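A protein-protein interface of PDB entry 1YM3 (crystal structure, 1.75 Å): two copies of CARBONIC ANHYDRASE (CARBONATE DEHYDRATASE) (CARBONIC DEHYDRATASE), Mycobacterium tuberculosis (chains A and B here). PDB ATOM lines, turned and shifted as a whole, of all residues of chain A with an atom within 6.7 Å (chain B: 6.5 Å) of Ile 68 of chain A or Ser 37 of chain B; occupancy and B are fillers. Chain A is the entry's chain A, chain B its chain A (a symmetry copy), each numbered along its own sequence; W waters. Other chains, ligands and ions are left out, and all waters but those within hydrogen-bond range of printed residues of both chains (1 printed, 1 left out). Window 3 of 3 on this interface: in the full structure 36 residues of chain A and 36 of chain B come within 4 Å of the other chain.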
ATOM      1  N   GLY A  24      32.284  12.325  -8.822  1.00  0.00           N
ATOM      2  CA  GLY A  24      31.106  12.458  -7.981  1.00  0.00           C
ATOM      3  C   GLY A  24      29.950  11.628  -8.505  1.00  0.00           C
ATOM      4  O   GLY A  24      29.253  10.979  -7.734  1.00  0.00           O
ATOM      5  N   ASN A  25      29.725  11.631  -9.823  1.00  0.00           N
ATOM      6  CA  ASN A  25      28.674  10.786 -10.360  1.00  0.00           C
ATOM      7  C   ASN A  25      28.974   9.257 -10.232  1.00  0.00           C
ATOM      8  O   ASN A  25      28.045   8.438 -10.040  1.00  0.00           O
ATOM      9  CB  ASN A  25      28.386  11.144 -11.804  1.00  0.00           C
ATOM     10  CG  ASN A  25      27.305  10.273 -12.398  1.00  0.00           C
ATOM     11  OD1 ASN A  25      27.586   9.431 -13.251  1.00  0.00           O
ATOM     12  ND2 ASN A  25      26.076  10.420 -11.905  1.00  0.00           N
ATOM     13  N   PHE A  28      27.847   8.463  -6.700  1.00  0.00           N
ATOM     14  CA  PHE A  28      26.378   8.383  -6.677  1.00  0.00           C
ATOM     15  C   PHE A  28      25.883   7.046  -7.229  1.00  0.00           C
ATOM     16  O   PHE A  28      25.073   6.353  -6.571  1.00  0.00           O
ATOM     17  CB  PHE A  28      25.757   9.582  -7.450  1.00  0.00           C
ATOM     18  CG  PHE A  28      24.266   9.492  -7.695  1.00  0.00           C
ATOM     19  CD1 PHE A  28      23.364   9.587  -6.651  1.00  0.00           C
ATOM     20  CD2 PHE A  28      23.772   9.338  -8.993  1.00  0.00           C
ATOM     21  CE1 PHE A  28      21.983   9.514  -6.890  1.00  0.00           C
ATOM     22  CE2 PHE A  28      22.425   9.273  -9.242  1.00  0.00           C
ATOM     23  CZ  PHE A  28      21.519   9.363  -8.190  1.00  0.00           C
ATOM     24  N   PRO A  33      27.946   7.834  -1.530  1.00  0.00           N
ATOM     25  CA  PRO A  33      28.189   9.276  -1.634  1.00  0.00           C
ATOM     26  C   PRO A  33      29.038   9.871  -0.508  1.00  0.00           C
ATOM     27  O   PRO A  33      28.853   9.491   0.639  1.00  0.00           O
ATOM     28  CB  PRO A  33      26.773   9.855  -1.605  1.00  0.00           C
ATOM     29  CG  PRO A  33      25.994   8.888  -0.780  1.00  0.00           C
ATOM     30  CD  PRO A  33      26.567   7.544  -1.101  1.00  0.00           C
ATOM     31  N   HIS A  35      28.991  13.270   0.015  1.00  0.00           N
ATOM     32  CA  HIS A  35      28.295  14.497   0.437  1.00  0.00           C
ATOM     33  C   HIS A  35      26.781  14.293   0.546  1.00  0.00           C
ATOM     34  O   HIS A  35      26.010  14.932  -0.201  1.00  0.00           O
ATOM     35  CB  HIS A  35      28.592  15.670  -0.530  1.00  0.00           C
ATOM     36  CG  HIS A  35      30.045  16.048  -0.632  1.00  0.00           C
ATOM     37  ND1 HIS A  35      30.768  16.526   0.438  1.00  0.00           N
ATOM     38  CD2 HIS A  35      30.892  16.064  -1.690  1.00  0.00           C
ATOM     39  CE1 HIS A  35      32.003  16.792   0.051  1.00  0.00           C
ATOM     40  NE2 HIS A  35      32.102  16.531  -1.238  1.00  0.00           N
ATOM     41  N   PRO A  36      26.339  13.437   1.481  1.00  0.00           N
ATOM     42  CA  PRO A  36      24.900  13.243   1.734  1.00  0.00           C
ATOM     43  C   PRO A  36      24.222  14.537   2.176  1.00  0.00           C
ATOM     44  O   PRO A  36      24.704  15.191   3.110  1.00  0.00           O
ATOM     45  CB  PRO A  36      24.861  12.194   2.860  1.00  0.00           C
ATOM     46  CG  PRO A  36      26.204  12.245   3.485  1.00  0.00           C
ATOM     47  CD  PRO A  36      27.164  12.608   2.376  1.00  0.00           C
ATOM     48  N   SER A  37      23.119  14.883   1.507  1.00  0.00           N
ATOM     49  CA  SER A  37      22.474  16.204   1.622  1.00  0.00           C
ATOM     50  C   SER A  37      23.477  17.367   1.479  1.00  0.00           C
ATOM     51  O   SER A  37      23.431  18.362   2.234  1.00  0.00           O
ATOM     52  CB  SER A  37      21.689  16.319   2.929  1.00  0.00           C
ATOM     53  OG  SER A  37      20.884  15.168   3.136  1.00  0.00           O
ATOM     54  N   GLN A  38      24.360  17.231   0.487  1.00  0.00           N
ATOM     55  CA  GLN A  38      25.438  18.194   0.215  1.00  0.00           C
ATOM     56  C   GLN A  38      26.355  18.459   1.420  1.00  0.00           C
ATOM     57  O   GLN A  38      27.023  19.502   1.475  1.00  0.00           O
ATOM     58  CB  GLN A  38      24.856  19.511  -0.356  1.00  0.00           C
ATOM     59  CG  GLN A  38      24.486  19.387  -1.832  1.00  0.00           C
ATOM     60  CD  GLN A  38      23.770  20.601  -2.363  1.00  0.00           C
ATOM     61  OE1 GLN A  38      22.551  20.582  -2.559  1.00  0.00           O
ATOM     62  NE2 GLN A  38      24.527  21.664  -2.614  1.00  0.00           N
ATOM     63  N   VAL A  64      15.300  15.319  -9.885  1.00  0.00           N
ATOM     64  CA  VAL A  64      16.398  15.187  -8.920  1.00  0.00           C
ATOM     65  C   VAL A  64      17.448  16.312  -9.069  1.00  0.00           C
ATOM     66  O   VAL A  64      17.793  16.688 -10.198  1.00  0.00           O
ATOM     67  CB  VAL A  64      17.060  13.807  -9.065  1.00  0.00           C
ATOM     68  CG1 VAL A  64      17.769  13.690 -10.360  1.00  0.00           C
ATOM     69  CG2 VAL A  64      18.020  13.498  -7.880  1.00  0.00           C
ATOM     70  N   ALA A  65      17.938  16.839  -7.939  1.00  0.00           N
ATOM     71  CA  ALA A  65      18.924  17.899  -7.936  1.00  0.00           C
ATOM     72  C   ALA A  65      20.248  17.428  -8.533  1.00  0.00           C
ATOM     73  O   ALA A  65      20.710  16.299  -8.268  1.00  0.00           O
ATOM     74  CB  ALA A  65      19.138  18.407  -6.572  1.00  0.00           C
ATOM     75  N   ALA A  66      20.844  18.266  -9.374  1.00  0.00           N
ATOM     76  CA  ALA A  66      22.176  17.976  -9.931  1.00  0.00           C
ATOM     77  C   ALA A  66      23.246  17.742  -8.853  1.00  0.00           C
ATOM     78  O   ALA A  66      24.145  16.995  -9.097  1.00  0.00           O
ATOM     79  CB  ALA A  66      22.634  19.065 -10.867  1.00  0.00           C
ATOM     80  N   GLU A  67      23.122  18.383  -7.691  1.00  0.00           N
ATOM     81  CA  GLU A  67      24.053  18.231  -6.558  1.00  0.00           C
ATOM     82  C   GLU A  67      24.082  16.783  -6.044  1.00  0.00           C
ATOM     83  O   GLU A  67      25.128  16.314  -5.542  1.00  0.00           O
ATOM     84  CB  GLU A  67      23.691  19.184  -5.410  1.00  0.00           C
ATOM     85  CG  GLU A  67      23.720  20.680  -5.775  1.00  0.00           C
ATOM     86  CD  GLU A  67      22.424  21.290  -6.390  1.00  0.00           C
ATOM     87  OE1 GLU A  67      21.569  20.593  -7.024  1.00  0.00           O
ATOM     88  OE2 GLU A  67      22.274  22.535  -6.274  1.00  0.00           O
ATOM     89  N   ILE A  68      22.952  16.083  -6.140  1.00  0.00           N
ATOM     90  CA  ILE A  68      22.873  14.661  -5.840  1.00  0.00           C
ATOM     91  C   ILE A  68      23.499  13.798  -6.958  1.00  0.00           C
ATOM     92  O   ILE A  68      24.277  12.880  -6.676  1.00  0.00           O
ATOM     93  CB  ILE A  68      21.377  14.233  -5.591  1.00  0.00           C
ATOM     94  CG1 ILE A  68      20.838  14.930  -4.341  1.00  0.00           C
ATOM     95  CG2 ILE A  68      21.227  12.689  -5.539  1.00  0.00           C
ATOM     96  CD1 ILE A  68      19.296  14.961  -4.231  1.00  0.00           C
ATOM     97  N   ILE A  69      23.128  14.055  -8.210  1.00  0.00           N
ATOM     98  CA  ILE A  69      23.586  13.276  -9.362  1.00  0.00           C
ATOM     99  C   ILE A  69      25.127  13.241  -9.420  1.00  0.00           C
ATOM    100  O   ILE A  69      25.743  12.213  -9.741  1.00  0.00           O
ATOM    101  CB  ILE A  69      23.048  13.964 -10.708  1.00  0.00           C
ATOM    102  CG1 ILE A  69      21.520  13.879 -10.847  1.00  0.00           C
ATOM    103  CG2 ILE A  69      23.731  13.382 -11.958  1.00  0.00           C
ATOM    104  CD1 ILE A  69      20.945  12.548 -10.575  1.00  0.00           C
ATOM    105  N   PHE A  70      25.740  14.378  -9.106  1.00  0.00           N
ATOM    106  CA  PHE A  70      27.189  14.563  -9.164  1.00  0.00           C
ATOM    107  C   PHE A  70      27.842  14.588  -7.758  1.00  0.00           C
ATOM    108  O   PHE A  70      29.023  14.887  -7.645  1.00  0.00           O
ATOM    109  CB  PHE A  70      27.528  15.867  -9.918  1.00  0.00           C
ATOM    110  CG  PHE A  70      27.192  15.837 -11.386  1.00  0.00           C
ATOM    111  CD1 PHE A  70      27.969  15.076 -12.256  1.00  0.00           C
ATOM    112  CD2 PHE A  70      26.110  16.558 -11.884  1.00  0.00           C
ATOM    113  CE1 PHE A  70      27.695  15.028 -13.587  1.00  0.00           C
ATOM    114  CE2 PHE A  70      25.787  16.499 -13.241  1.00  0.00           C
ATOM    115  CZ  PHE A  70      26.580  15.731 -14.111  1.00  0.00           C
ATOM    116  N   ASP A  71      27.084  14.278  -6.703  1.00  0.00           N
ATOM    117  CA  ASP A  71      27.621  14.162  -5.336  1.00  0.00           C
ATOM    118  C   ASP A  71      28.582  15.274  -4.929  1.00  0.00           C
ATOM    119  O   ASP A  71      29.762  15.021  -4.638  1.00  0.00           O
ATOM    120  CB  ASP A  71      28.317  12.811  -5.157  1.00  0.00           C
ATOM    121  CG  ASP A  71      28.674  12.538  -3.735  1.00  0.00           C
ATOM    122  OD1 ASP A  71      27.860  12.870  -2.855  1.00  0.00           O
ATOM    123  OD2 ASP A  71      29.751  12.045  -3.397  1.00  0.00           O
ATOM    124  N   GLN A  72      28.061  16.507  -4.933  1.00  0.00           N
ATOM    125  CA  GLN A  72      28.822  17.721  -4.653  1.00  0.00           C
ATOM    126  C   GLN A  72      28.344  18.278  -3.327  1.00  0.00           C
ATOM    127  O   GLN A  72      27.235  17.947  -2.906  1.00  0.00           O
ATOM    128  CB  GLN A  72      28.585  18.743  -5.773  1.00  0.00           C
ATOM    129  CG  GLN A  72      29.051  18.250  -7.113  1.00  0.00           C
ATOM    130  CD  GLN A  72      30.522  18.152  -7.169  1.00  0.00           C
ATOM    131  OE1 GLN A  72      31.193  19.179  -7.133  1.00  0.00           O
ATOM    132  NE2 GLN A  72      31.060  16.931  -7.247  1.00  0.00           N
ATOM    133  N   MET A  77      28.245  24.186  -6.961  1.00  0.00           N
ATOM    134  CA  MET A  77      27.530  24.298  -8.227  1.00  0.00           C
ATOM    135  C   MET A  77      26.733  25.622  -8.293  1.00  0.00           C
ATOM    136  O   MET A  77      26.101  26.009  -7.305  1.00  0.00           O
ATOM    137  CB  MET A  77      26.590  23.089  -8.394  1.00  0.00           C
ATOM    138  CG  MET A  77      27.332  21.716  -8.474  1.00  0.00           C
ATOM    139  SD  MET A  77      26.286  20.312  -9.006  1.00  0.00           S
ATOM    140  CE  MET A  77      24.884  21.157  -9.349  1.00  0.00           C
ATOM    141  N   HIS B  35      13.336  12.269   3.541  1.00  0.00           N
ATOM    142  CA  HIS B  35      13.750  12.028   2.149  1.00  0.00           C
ATOM    143  C   HIS B  35      15.230  12.350   1.924  1.00  0.00           C
ATOM    144  O   HIS B  35      15.557  13.267   1.140  1.00  0.00           O
ATOM    145  CB  HIS B  35      12.884  12.845   1.158  1.00  0.00           C
ATOM    146  CG  HIS B  35      11.414  12.530   1.199  1.00  0.00           C
ATOM    147  ND1 HIS B  35      10.909  11.289   0.878  1.00  0.00           N
ATOM    148  CD2 HIS B  35      10.340  13.309   1.475  1.00  0.00           C
ATOM    149  CE1 HIS B  35       9.592  11.310   0.983  1.00  0.00           C
ATOM    150  NE2 HIS B  35       9.220  12.527   1.332  1.00  0.00           N
ATOM    151  N   PRO B  36      16.131  11.596   2.572  1.00  0.00           N
ATOM    152  CA  PRO B  36      17.580  11.759   2.350  1.00  0.00           C
ATOM    153  C   PRO B  36      17.965  11.492   0.897  1.00  0.00           C
ATOM    154  O   PRO B  36      17.595  10.446   0.349  1.00  0.00           O
ATOM    155  CB  PRO B  36      18.217  10.714   3.284  1.00  0.00           C
ATOM    156  CG  PRO B  36      17.137   9.738   3.568  1.00  0.00           C
ATOM    157  CD  PRO B  36      15.848  10.527   3.545  1.00  0.00           C
ATOM    158  N   SER B  37      18.700  12.434   0.300  1.00  0.00           N
ATOM    159  CA  SER B  37      18.957  12.472  -1.151  1.00  0.00           C
ATOM    160  C   SER B  37      17.671  12.302  -1.986  1.00  0.00           C
ATOM    161  O   SER B  37      17.643  11.565  -2.995  1.00  0.00           O
ATOM    162  CB  SER B  37      20.006  11.433  -1.550  1.00  0.00           C
ATOM    163  OG  SER B  37      21.124  11.486  -0.677  1.00  0.00           O
ATOM    164  N   GLN B  38      16.624  13.011  -1.558  1.00  0.00           N
ATOM    165  CA  GLN B  38      15.288  12.949  -2.172  1.00  0.00           C
ATOM    166  C   GLN B  38      14.701  11.530  -2.242  1.00  0.00           C
ATOM    167  O   GLN B  38      13.811  11.266  -3.063  1.00  0.00           O
ATOM    168  CB  GLN B  38      15.301  13.628  -3.564  1.00  0.00           C
ATOM    169  CG  GLN B  38      15.271  15.151  -3.464  1.00  0.00           C
ATOM    170  CD  GLN B  38      15.447  15.831  -4.796  1.00  0.00           C
ATOM    171  OE1 GLN B  38      16.520  16.359  -5.102  1.00  0.00           O
ATOM    172  NE2 GLN B  38      14.385  15.836  -5.595  1.00  0.00           N
ATOM    173  N   SER B  39      15.146  10.668  -1.313  1.00  0.00           N
ATOM    174  CA  SER B  39      14.904   9.215  -1.338  1.00  0.00           C
ATOM    175  C   SER B  39      15.356   8.605  -2.671  1.00  0.00           C
ATOM    176  O   SER B  39      14.769   7.631  -3.157  1.00  0.00           O
ATOM    177  CB  SER B  39      13.425   8.875  -1.069  1.00  0.00           C
ATOM    178  OG  SER B  39      12.930   9.531   0.088  1.00  0.00           O
ATOM    179  N   ALA B  65      20.335  22.900  -2.473  1.00  0.00           N
ATOM    180  CA  ALA B  65      19.133  22.597  -3.220  1.00  0.00           C
ATOM    181  C   ALA B  65      17.881  22.812  -2.372  1.00  0.00           C
ATOM    182  O   ALA B  65      17.843  22.456  -1.176  1.00  0.00           O
ATOM    183  CB  ALA B  65      19.167  21.216  -3.725  1.00  0.00           C
ATOM    184  N   GLU B  67      15.200  21.180  -2.547  1.00  0.00           N
ATOM    185  CA  GLU B  67      14.697  19.836  -2.209  1.00  0.00           C
ATOM    186  C   GLU B  67      15.214  19.370  -0.840  1.00  0.00           C
ATOM    187  O   GLU B  67      14.520  18.608  -0.131  1.00  0.00           O
ATOM    188  CB  GLU B  67      15.079  18.812  -3.288  1.00  0.00           C
ATOM    189  CG  GLU B  67      14.535  19.119  -4.696  1.00  0.00           C
ATOM    190  CD  GLU B  67      15.390  20.056  -5.603  1.00  0.00           C
ATOM    191  OE1 GLU B  67      16.197  20.920  -5.133  1.00  0.00           O
ATOM    192  OE2 GLU B  67      15.213  19.957  -6.845  1.00  0.00           O
ATOM    193  N   ILE B  68      16.423  19.793  -0.473  1.00  0.00           N
ATOM    194  CA  ILE B  68      16.975  19.562   0.854  1.00  0.00           C
ATOM    195  C   ILE B  68      16.332  20.481   1.916  1.00  0.00           C
ATOM    196  O   ILE B  68      15.949  20.016   2.996  1.00  0.00           O
ATOM    197  CB  ILE B  68      18.539  19.750   0.842  1.00  0.00           C
ATOM    198  CG1 ILE B  68      19.183  18.683  -0.046  1.00  0.00           C
ATOM    199  CG2 ILE B  68      19.121  19.779   2.279  1.00  0.00           C
ATOM    200  CD1 ILE B  68      20.624  19.007  -0.504  1.00  0.00           C
ATOM    201  N   GLN B  72      11.934  17.201   0.454  1.00  0.00           N
ATOM    202  CA  GLN B  72      10.971  16.691  -0.519  1.00  0.00           C
ATOM    203  C   GLN B  72      11.620  15.538  -1.258  1.00  0.00           C
ATOM    204  O   GLN B  72      12.848  15.450  -1.268  1.00  0.00           O
ATOM    205  CB  GLN B  72      10.598  17.808  -1.503  1.00  0.00           C
ATOM    206  CG  GLN B  72       9.939  18.977  -0.827  1.00  0.00           C
ATOM    207  CD  GLN B  72       8.597  18.623  -0.327  1.00  0.00           C
ATOM    208  OE1 GLN B  72       7.703  18.377  -1.131  1.00  0.00           O
ATOM    209  NE2 GLN B  72       8.420  18.576   0.997  1.00  0.00           N
ATOM    210  N   LEU B  74      11.317  12.770  -4.964  1.00  0.00           N
ATOM    211  CA  LEU B  74      11.525  12.920  -6.404  1.00  0.00           C
ATOM    212  C   LEU B  74      10.309  13.439  -7.127  1.00  0.00           C
ATOM    213  O   LEU B  74       9.215  12.869  -7.013  1.00  0.00           O
ATOM    214  CB  LEU B  74      11.892  11.577  -7.027  1.00  0.00           C
ATOM    215  CG  LEU B  74      13.233  10.972  -6.630  1.00  0.00           C
ATOM    216  CD1 LEU B  74      13.354   9.648  -7.295  1.00  0.00           C
ATOM    217  CD2 LEU B  74      14.410  11.891  -7.031  1.00  0.00           C
HETATM  218  O   HOH W   1      14.261  18.023  -7.988  1.00  0.00           O
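Ser 37 of chain A touches Ile 68 of chain B, and with the chains exchanged Ile 68 of chain A touches Ser 37 of chain B. Gln 38 of chain A touches Ala 65 of chain B, and with the chains exchanged Ala 65 of chain A touches Gln 38 of chain B. Gln 38 of chain A touches Ile 68 of chain B, and with the chains exchanged Ile 68 of chain A touches Gln 38 of chain B. Ala 65 of chain B touches its own counterpart, Ala 65 of chain A. Of the 9 pairs that touch across the chains among the printed residues, 7 have their exchanged pair printed and touching as well.
The side-chain amide oxygen (OE1) of Gln 38 of chain B lies within hydrogen-bond range of the backbone NH (N) of Ala 65 of chain A (3.2 Å). The side-chain amide oxygen (OE1) of Gln 38 of chain A sits at hydrogen-bond distance from the backbone NH (N) of Ala 65 of chain B.
Of chain B, only Ser 37 and Gln 38 come within 4 Å of Ile 68 of chain A. Ser 37 of chain B touches one residue of chain A. Of the printed residues of chain B, Val 64 of chain A touches Gln 38 and Leu 74. Of the printed residues of chain A, Gln 38 of chain B touches Val 64 (3.9 Å), Ala 65 (3.2 Å) and Ile 68 (3.2 Å). The nearest residue of chain A that does not touch Ser 37 of chain B is Ser 37 of chain A (4.5 Å). The nearest printed residue of chain A that does not touch Leu 74 of chain B is Ala 65 of chain A (6.1 Å).
The backbone carbonyl oxygen (O) of Gln 38 of chain B sits at hydrogen-bond distance from the backbone NH (N) of Leu 74 of chain B, 3.5 Å away.
Water W1 lies within hydrogen-bond range of the side-chain carboxylate (OE2) of Glu 67 of chain B (2.4 Å), the side-chain amide nitrogen (NE2) of Gln 38 of chain B (3.2 Å) and the backbone NH (N) of Val 64 of chain A (3.5 Å).
Ile 68 of chain B touches Ser 37 of chain A (CD1 to C, 3.8 Å). Ile 68 of chain B touches Gln 38 of chain A. Val 64 of chain A touches Gln 38 of chain B. Leu 74 of chain B touches Val 64 of chain A. Ala 65 of chain B touches Ala 65 of chain A (CB to CB, 3.9996 Å). C of Ser 37 of chain B touches CD1 of Ile 68 of chain A (3.8 Å). Gln 38 of chain B touches Ile 68 of chain A (OE1 to CD1, 3.2 Å).
Of the 10 printed residues of chain B, 5 touch a printed residue of chain A. Among the printed residues, 9 pairs touch across the chains. Among the printed residues, no Asp or Glu carboxylate lies within 4 Å of a Lys or Arg side-chain nitrogen of the other chain.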
